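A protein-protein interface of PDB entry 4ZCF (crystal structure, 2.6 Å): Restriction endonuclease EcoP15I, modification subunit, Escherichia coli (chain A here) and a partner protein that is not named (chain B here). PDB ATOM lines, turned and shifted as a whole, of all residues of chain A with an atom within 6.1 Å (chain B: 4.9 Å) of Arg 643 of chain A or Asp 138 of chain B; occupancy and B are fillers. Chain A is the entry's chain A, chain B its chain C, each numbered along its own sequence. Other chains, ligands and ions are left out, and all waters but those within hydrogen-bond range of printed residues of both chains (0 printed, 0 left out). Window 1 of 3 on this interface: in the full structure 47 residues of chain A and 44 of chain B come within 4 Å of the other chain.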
ATOM      1  N   TRP A 549       3.711  13.525  10.164  1.00  0.00           N
ATOM      2  CA  TRP A 549       5.081  13.220  10.543  1.00  0.00           C
ATOM      3  C   TRP A 549       5.369  11.743  10.495  1.00  0.00           C
ATOM      4  O   TRP A 549       6.416  11.374   9.999  1.00  0.00           O
ATOM      5  CB  TRP A 549       5.415  13.780  11.935  1.00  0.00           C
ATOM      6  CG  TRP A 549       5.619  15.266  11.998  1.00  0.00           C
ATOM      7  CD1 TRP A 549       5.300  16.194  11.046  1.00  0.00           C
ATOM      8  CD2 TRP A 549       6.139  15.995  13.112  1.00  0.00           C
ATOM      9  NE1 TRP A 549       5.598  17.457  11.498  1.00  0.00           N
ATOM     10  CE2 TRP A 549       6.083  17.368  12.779  1.00  0.00           C
ATOM     11  CE3 TRP A 549       6.667  15.620  14.365  1.00  0.00           C
ATOM     12  CZ2 TRP A 549       6.547  18.369  13.650  1.00  0.00           C
ATOM     13  CZ3 TRP A 549       7.107  16.609  15.231  1.00  0.00           C
ATOM     14  CH2 TRP A 549       7.065  17.962  14.867  1.00  0.00           C
ATOM     15  N   CYS A 550       4.452  10.892  11.000  1.00  0.00           N
ATOM     16  CA  CYS A 550       4.621   9.434  10.980  1.00  0.00           C
ATOM     17  C   CYS A 550       4.701   8.881   9.539  1.00  0.00           C
ATOM     18  O   CYS A 550       5.450   7.943   9.297  1.00  0.00           O
ATOM     19  CB  CYS A 550       3.510   8.754  11.774  1.00  0.00           C
ATOM     20  SG  CYS A 550       3.765   8.750  13.569  1.00  0.00           S
ATOM     21  N   TYR A 552       5.419  10.823   6.601  1.00  0.00           N
ATOM     22  CA  TYR A 552       6.617  11.466   6.071  1.00  0.00           C
ATOM     23  C   TYR A 552       7.875  10.691   6.498  1.00  0.00           C
ATOM     24  O   TYR A 552       8.765  10.489   5.685  1.00  0.00           O
ATOM     25  CB  TYR A 552       6.690  12.945   6.532  1.00  0.00           C
ATOM     26  CG  TYR A 552       7.977  13.626   6.117  1.00  0.00           C
ATOM     27  CD1 TYR A 552       8.115  14.185   4.849  1.00  0.00           C
ATOM     28  CD2 TYR A 552       9.092  13.626   6.955  1.00  0.00           C
ATOM     29  CE1 TYR A 552       9.323  14.742   4.431  1.00  0.00           C
ATOM     30  CE2 TYR A 552      10.306  14.162   6.541  1.00  0.00           C
ATOM     31  CZ  TYR A 552      10.409  14.747   5.289  1.00  0.00           C
ATOM     32  OH  TYR A 552      11.588  15.319   4.882  1.00  0.00           O
ATOM     33  N   ASP A 553       7.922  10.235   7.761  1.00  0.00           N
ATOM     34  CA  ASP A 553       9.022   9.472   8.350  1.00  0.00           C
ATOM     35  C   ASP A 553       9.151   8.048   7.818  1.00  0.00           C
ATOM     36  O   ASP A 553      10.095   7.357   8.192  1.00  0.00           O
ATOM     37  CB  ASP A 553       8.984   9.513   9.902  1.00  0.00           C
ATOM     38  CG  ASP A 553       9.525  10.803  10.520  1.00  0.00           C
ATOM     39  OD1 ASP A 553      10.599  11.267  10.082  1.00  0.00           O
ATOM     40  OD2 ASP A 553       8.916  11.299  11.484  1.00  0.00           O
ATOM     41  N   TYR A 579       8.001  10.507  19.222  1.00  0.00           N
ATOM     42  CA  TYR A 579       7.564  11.886  18.993  1.00  0.00           C
ATOM     43  C   TYR A 579       7.270  12.681  20.258  1.00  0.00           C
ATOM     44  O   TYR A 579       6.484  12.253  21.103  1.00  0.00           O
ATOM     45  CB  TYR A 579       6.365  11.922  18.023  1.00  0.00           C
ATOM     46  CG  TYR A 579       6.686  11.297  16.687  1.00  0.00           C
ATOM     47  CD1 TYR A 579       6.667   9.911  16.518  1.00  0.00           C
ATOM     48  CD2 TYR A 579       7.067  12.082  15.604  1.00  0.00           C
ATOM     49  CE1 TYR A 579       6.997   9.327  15.295  1.00  0.00           C
ATOM     50  CE2 TYR A 579       7.406  11.508  14.381  1.00  0.00           C
ATOM     51  CZ  TYR A 579       7.374  10.131  14.234  1.00  0.00           C
ATOM     52  OH  TYR A 579       7.713   9.566  13.037  1.00  0.00           O
ATOM     53  N   LYS A 607      15.275   6.545  17.248  1.00  0.00           N
ATOM     54  CA  LYS A 607      15.141   7.886  16.697  1.00  0.00           C
ATOM     55  C   LYS A 607      14.155   8.656  17.590  1.00  0.00           C
ATOM     56  O   LYS A 607      13.128   8.096  17.995  1.00  0.00           O
ATOM     57  CB  LYS A 607      14.613   7.768  15.245  1.00  0.00           C
ATOM     58  CG  LYS A 607      14.810   8.992  14.368  1.00  0.00           C
ATOM     59  CD  LYS A 607      14.070   8.790  13.043  1.00  0.00           C
ATOM     60  CE  LYS A 607      13.425  10.054  12.530  1.00  0.00           C
ATOM     61  NZ  LYS A 607      12.330   9.776  11.577  1.00  0.00           N
ATOM     62  N   VAL A 609      12.104  12.336  17.675  1.00  0.00           N
ATOM     63  CA  VAL A 609      11.638  13.502  16.901  1.00  0.00           C
ATOM     64  C   VAL A 609      10.830  14.441  17.825  1.00  0.00           C
ATOM     65  O   VAL A 609       9.870  14.007  18.442  1.00  0.00           O
ATOM     66  CB  VAL A 609      10.825  13.096  15.628  1.00  0.00           C
ATOM     67  CG1 VAL A 609      10.636  14.273  14.672  1.00  0.00           C
ATOM     68  CG2 VAL A 609      11.454  11.913  14.910  1.00  0.00           C
ATOM     69  N   PHE A 610      11.221  15.707  17.922  1.00  0.00           N
ATOM     70  CA  PHE A 610      10.502  16.657  18.776  1.00  0.00           C
ATOM     71  C   PHE A 610      10.119  17.938  18.029  1.00  0.00           C
ATOM     72  O   PHE A 610      10.824  18.361  17.115  1.00  0.00           O
ATOM     73  CB  PHE A 610      11.290  16.960  20.077  1.00  0.00           C
ATOM     74  CG  PHE A 610      12.567  17.742  19.867  1.00  0.00           C
ATOM     75  CD1 PHE A 610      13.763  17.091  19.584  1.00  0.00           C
ATOM     76  CD2 PHE A 610      12.564  19.132  19.903  1.00  0.00           C
ATOM     77  CE1 PHE A 610      14.927  17.817  19.322  1.00  0.00           C
ATOM     78  CE2 PHE A 610      13.736  19.853  19.661  1.00  0.00           C
ATOM     79  CZ  PHE A 610      14.906  19.188  19.369  1.00  0.00           C
ATOM     80  N   TYR A 611       9.001  18.546  18.420  1.00  0.00           N
ATOM     81  CA  TYR A 611       8.516  19.788  17.822  1.00  0.00           C
ATOM     82  C   TYR A 611       9.271  21.024  18.393  1.00  0.00           C
ATOM     83  O   TYR A 611       9.037  21.421  19.536  1.00  0.00           O
ATOM     84  CB  TYR A 611       6.997  19.878  18.039  1.00  0.00           C
ATOM     85  CG  TYR A 611       6.315  21.084  17.449  1.00  0.00           C
ATOM     86  CD1 TYR A 611       6.667  21.563  16.193  1.00  0.00           C
ATOM     87  CD2 TYR A 611       5.247  21.687  18.096  1.00  0.00           C
ATOM     88  CE1 TYR A 611       6.024  22.669  15.633  1.00  0.00           C
ATOM     89  CE2 TYR A 611       4.613  22.807  17.560  1.00  0.00           C
ATOM     90  CZ  TYR A 611       4.997  23.288  16.320  1.00  0.00           C
ATOM     91  OH  TYR A 611       4.338  24.358  15.760  1.00  0.00           O
ATOM     92  N   GLY A 612      10.159  21.598  17.569  1.00  0.00           N
ATOM     93  CA  GLY A 612      11.001  22.764  17.839  1.00  0.00           C
ATOM     94  C   GLY A 612      10.362  23.908  18.599  1.00  0.00           C
ATOM     95  O   GLY A 612      10.867  24.290  19.658  1.00  0.00           O
ATOM     96  N   SER A 613       9.222  24.434  18.087  1.00  0.00           N
ATOM     97  CA  SER A 613       8.452  25.543  18.684  1.00  0.00           C
ATOM     98  C   SER A 613       8.073  25.344  20.165  1.00  0.00           C
ATOM     99  O   SER A 613       7.959  26.331  20.902  1.00  0.00           O
ATOM    100  CB  SER A 613       7.192  25.815  17.871  1.00  0.00           C
ATOM    101  OG  SER A 613       7.384  26.887  16.962  1.00  0.00           O
ATOM    102  N   ASP A 639      19.172   8.714  17.766  1.00  0.00           N
ATOM    103  CA  ASP A 639      19.294   9.956  16.995  1.00  0.00           C
ATOM    104  C   ASP A 639      18.212  10.936  17.439  1.00  0.00           C
ATOM    105  O   ASP A 639      17.129  10.508  17.855  1.00  0.00           O
ATOM    106  CB  ASP A 639      19.200   9.724  15.480  1.00  0.00           C
ATOM    107  CG  ASP A 639      19.664  10.921  14.650  1.00  0.00           C
ATOM    108  OD1 ASP A 639      20.796  11.425  14.899  1.00  0.00           O
ATOM    109  OD2 ASP A 639      18.903  11.353  13.746  1.00  0.00           O
ATOM    110  N   VAL A 641      16.084  14.286  16.166  1.00  0.00           N
ATOM    111  CA  VAL A 641      15.621  15.119  15.053  1.00  0.00           C
ATOM    112  C   VAL A 641      14.737  16.284  15.527  1.00  0.00           C
ATOM    113  O   VAL A 641      13.950  16.101  16.460  1.00  0.00           O
ATOM    114  CB  VAL A 641      14.893  14.199  14.018  1.00  0.00           C
ATOM    115  CG1 VAL A 641      14.400  14.973  12.794  1.00  0.00           C
ATOM    116  CG2 VAL A 641      15.783  13.038  13.589  1.00  0.00           C
ATOM    117  N   VAL A 642      14.869  17.469  14.872  1.00  0.00           N
ATOM    118  CA  VAL A 642      14.060  18.684  15.067  1.00  0.00           C
ATOM    119  C   VAL A 642      13.101  18.854  13.872  1.00  0.00           C
ATOM    120  O   VAL A 642      13.536  18.817  12.707  1.00  0.00           O
ATOM    121  CB  VAL A 642      14.854  20.017  15.208  1.00  0.00           C
ATOM    122  CG1 VAL A 642      14.158  20.964  16.187  1.00  0.00           C
ATOM    123  CG2 VAL A 642      16.313  19.808  15.576  1.00  0.00           C
ATOM    124  N   ARG A 643      11.828  19.163  14.164  1.00  0.00           N
ATOM    125  CA  ARG A 643      10.846  19.414  13.116  1.00  0.00           C
ATOM    126  C   ARG A 643       9.960  20.613  13.462  1.00  0.00           C
ATOM    127  O   ARG A 643       9.394  20.660  14.555  1.00  0.00           O
ATOM    128  CB  ARG A 643      10.020  18.147  12.810  1.00  0.00           C
ATOM    129  CG  ARG A 643       9.382  18.173  11.426  1.00  0.00           C
ATOM    130  CD  ARG A 643       8.950  16.804  10.962  1.00  0.00           C
ATOM    131  NE  ARG A 643      10.090  15.914  10.811  1.00  0.00           N
ATOM    132  CZ  ARG A 643      10.039  14.598  10.945  1.00  0.00           C
ATOM    133  NH1 ARG A 643       8.897  14.000  11.264  1.00  0.00           N
ATOM    134  NH2 ARG A 643      11.132  13.869  10.785  1.00  0.00           N
ATOM    135  N   ASN A 644       9.836  21.573  12.514  1.00  0.00           N
ATOM    136  CA  ASN A 644       9.069  22.826  12.624  1.00  0.00           C
ATOM    137  C   ASN A 644       9.433  23.664  13.861  1.00  0.00           C
ATOM    138  O   ASN A 644      10.564  23.616  14.344  1.00  0.00           O
ATOM    139  CB  ASN A 644       7.557  22.582  12.551  1.00  0.00           C
ATOM    140  CG  ASN A 644       6.994  22.458  11.160  1.00  0.00           C
ATOM    141  OD1 ASN A 644       6.641  21.364  10.698  1.00  0.00           O
ATOM    142  ND2 ASN A 644       6.830  23.590  10.489  1.00  0.00           N
ATOM    143  N   GLU B 134      15.667   6.821   5.637  1.00  0.00           N
ATOM    144  CA  GLU B 134      15.373   7.553   6.875  1.00  0.00           C
ATOM    145  C   GLU B 134      16.595   8.285   7.368  1.00  0.00           C
ATOM    146  O   GLU B 134      16.483   9.470   7.625  1.00  0.00           O
ATOM    147  CB  GLU B 134      14.813   6.636   7.959  1.00  0.00           C
ATOM    148  CG  GLU B 134      13.318   6.443   7.835  1.00  0.00           C
ATOM    149  CD  GLU B 134      12.803   5.127   8.381  1.00  0.00           C
ATOM    150  OE1 GLU B 134      13.147   4.788   9.538  1.00  0.00           O
ATOM    151  OE2 GLU B 134      12.055   4.433   7.652  1.00  0.00           O
ATOM    152  N   HIS B 135      17.769   7.613   7.421  1.00  0.00           N
ATOM    153  CA  HIS B 135      19.054   8.193   7.832  1.00  0.00           C
ATOM    154  C   HIS B 135      19.379   9.473   7.057  1.00  0.00           C
ATOM    155  O   HIS B 135      19.615  10.509   7.670  1.00  0.00           O
ATOM    156  CB  HIS B 135      20.192   7.157   7.697  1.00  0.00           C
ATOM    157  CG  HIS B 135      21.560   7.684   8.024  1.00  0.00           C
ATOM    158  ND1 HIS B 135      21.991   7.810   9.326  1.00  0.00           N
ATOM    159  CD2 HIS B 135      22.558   8.079   7.192  1.00  0.00           C
ATOM    160  CE1 HIS B 135      23.220   8.294   9.249  1.00  0.00           C
ATOM    161  NE2 HIS B 135      23.603   8.462   7.986  1.00  0.00           N
ATOM    162  N   PHE B 136      19.333   9.412   5.722  1.00  0.00           N
ATOM    163  CA  PHE B 136      19.653  10.549   4.858  1.00  0.00           C
ATOM    164  C   PHE B 136      18.598  11.637   4.677  1.00  0.00           C
ATOM    165  O   PHE B 136      18.966  12.754   4.312  1.00  0.00           O
ATOM    166  CB  PHE B 136      20.259  10.093   3.533  1.00  0.00           C
ATOM    167  CG  PHE B 136      21.670   9.570   3.645  1.00  0.00           C
ATOM    168  CD1 PHE B 136      22.718  10.416   4.008  1.00  0.00           C
ATOM    169  CD2 PHE B 136      21.965   8.250   3.326  1.00  0.00           C
ATOM    170  CE1 PHE B 136      24.029   9.939   4.086  1.00  0.00           C
ATOM    171  CE2 PHE B 136      23.280   7.777   3.391  1.00  0.00           C
ATOM    172  CZ  PHE B 136      24.305   8.628   3.766  1.00  0.00           C
ATOM    173  N   ARG B 137      17.316  11.340   4.954  1.00  0.00           N
ATOM    174  CA  ARG B 137      16.212  12.320   4.883  1.00  0.00           C
ATOM    175  C   ARG B 137      16.263  13.192   6.140  1.00  0.00           C
ATOM    176  O   ARG B 137      15.973  14.384   6.083  1.00  0.00           O
ATOM    177  CB  ARG B 137      14.852  11.597   4.774  1.00  0.00           C
ATOM    178  CG  ARG B 137      13.609  12.495   4.648  1.00  0.00           C
ATOM    179  CD  ARG B 137      12.357  11.744   4.199  1.00  0.00           C
ATOM    180  NE  ARG B 137      12.130  10.531   4.975  1.00  0.00           N
ATOM    181  CZ  ARG B 137      12.118   9.302   4.469  1.00  0.00           C
ATOM    182  NH1 ARG B 137      12.301   9.108   3.163  1.00  0.00           N
ATOM    183  NH2 ARG B 137      11.919   8.258   5.259  1.00  0.00           N
ATOM    184  N   ASP B 138      16.642  12.594   7.276  1.00  0.00           N
ATOM    185  CA  ASP B 138      16.777  13.323   8.527  1.00  0.00           C
ATOM    186  C   ASP B 138      17.941  14.324   8.432  1.00  0.00           C
ATOM    187  O   ASP B 138      17.752  15.521   8.679  1.00  0.00           O
ATOM    188  CB  ASP B 138      17.010  12.353   9.695  1.00  0.00           C
ATOM    189  CG  ASP B 138      15.775  11.624  10.198  1.00  0.00           C
ATOM    190  OD1 ASP B 138      14.651  12.173  10.043  1.00  0.00           O
ATOM    191  OD2 ASP B 138      15.935  10.523  10.782  1.00  0.00           O
ATOM    192  N   ASP B 139      19.120  13.831   8.041  1.00  0.00           N
ATOM    193  CA  ASP B 139      20.341  14.606   7.980  1.00  0.00           C
ATOM    194  C   ASP B 139      20.426  15.627   6.849  1.00  0.00           C
ATOM    195  O   ASP B 139      21.116  16.627   7.024  1.00  0.00           O
ATOM    196  CB  ASP B 139      21.562  13.672   7.975  1.00  0.00           C
ATOM    197  CG  ASP B 139      21.829  12.888   9.258  1.00  0.00           C
ATOM    198  OD1 ASP B 139      21.268  13.265  10.321  1.00  0.00           O
ATOM    199  OD2 ASP B 139      22.648  11.932   9.212  1.00  0.00           O
ATOM    200  N   TYR B 140      19.741  15.395   5.702  1.00  0.00           N
ATOM    201  CA  TYR B 140      19.830  16.285   4.528  1.00  0.00           C
ATOM    202  C   TYR B 140      18.541  16.831   3.943  1.00  0.00           C
ATOM    203  O   TYR B 140      18.614  17.752   3.123  1.00  0.00           O
ATOM    204  CB  TYR B 140      20.624  15.597   3.394  1.00  0.00           C
ATOM    205  CG  TYR B 140      22.073  15.318   3.736  1.00  0.00           C
ATOM    206  CD1 TYR B 140      22.446  14.133   4.368  1.00  0.00           C
ATOM    207  CD2 TYR B 140      23.066  16.251   3.459  1.00  0.00           C
ATOM    208  CE1 TYR B 140      23.770  13.886   4.722  1.00  0.00           C
ATOM    209  CE2 TYR B 140      24.399  15.990   3.754  1.00  0.00           C
ATOM    210  CZ  TYR B 140      24.746  14.812   4.401  1.00  0.00           C
ATOM    211  OH  TYR B 140      26.055  14.550   4.713  1.00  0.00           O
ATOM    212  N   LYS B 141      17.364  16.263   4.321  1.00  0.00           N
ATOM    213  CA  LYS B 141      16.047  16.599   3.759  1.00  0.00           C
ATOM    214  C   LYS B 141      16.101  16.370   2.233  1.00  0.00           C
ATOM    215  O   LYS B 141      15.655  17.198   1.434  1.00  0.00           O
ATOM    216  CB  LYS B 141      15.638  18.028   4.119  1.00  0.00           C
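O of Tyr 552 of chain A is in hydrogen-bond range of NE of Arg 137 of chain B, at 3.4 Å.
NZ of Lys 607 of chain A lies within salt-bridge range of OD1 of Asp 138 of chain B.
The guanidinium group (NH2) of Arg 643 of chain A lies within salt-bridge range of the side-chain carboxylate (OD1) of Asp 138 of chain B (3.98 Å).
The side-chain carboxylate (OD2) of Asp 553 of chain A sits at hydrogen-bond distance from the side-chain hydroxyl (OH) of Tyr 579 of chain A, 2.6 Å away.
The side-chain carboxylate of Asp 553 of chain A is in salt-bridge range of the side-chain amino group of Lys 607 of chain A (2.7 Å).
OD2 of Asp 553 of chain A is in salt-bridge range of NH1 of Arg 643 of chain A.
The backbone NH of Phe 610 of chain A lies within hydrogen-bond range of the backbone carbonyl oxygen of Val 641 of chain A (3.1 Å).
The backbone carbonyl oxygen (O) of Phe 610 of chain A sits at hydrogen-bond distance from the backbone NH (N) of Arg 643 of chain A.
N of Gly 612 of chain A lies within hydrogen-bond range of O of Arg 643 of chain A, 3.2 Å away.
Among the printed residues, pairs that only touch across the chains: Asp 553 of chain A with Glu 134 of chain B (3.4 Å), Asp 553 of chain A with Arg 137 of chain B (3.6 Å) and Val 641 of chain A with Asp 138 of chain B (3.7 Å).
Of chain B, only Asp 138 comes within 4 Å of Arg 643 of chain A.
Asp 138 of chain B touches three residues of chain A.
Printed residues of chain B within 4 Å of Tyr 552 of chain A: Arg 137 (3.4 Å).
Printed residues of chain A within 4 Å of Arg 137 of chain B: Tyr 552 (3.4 Å) and Asp 553 (3.6 Å).
Gly 612 of chain A touches none of the printed residues of chain B.
The nearest residue of chain A that does not touch Asp 138 of chain B is Asp 553 of chain A (4.2 Å).
The nearest printed residue of chain B that does not touch Lys 607 of chain A is Glu 134 of chain B (5.1 Å).
Of the 16 printed residues of chain A, 5 touch a printed residue of chain B.
Printed residues of chain A that touch a printed residue of chain B: Tyr 552, Asp 553, Lys 607, Val 641 and Arg 643.
Of the 8 printed residues of chain B, 3 touch a printed residue of chain A.
Along chain B the printed residues that touch a printed residue of chain A span positions 134 to 138.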
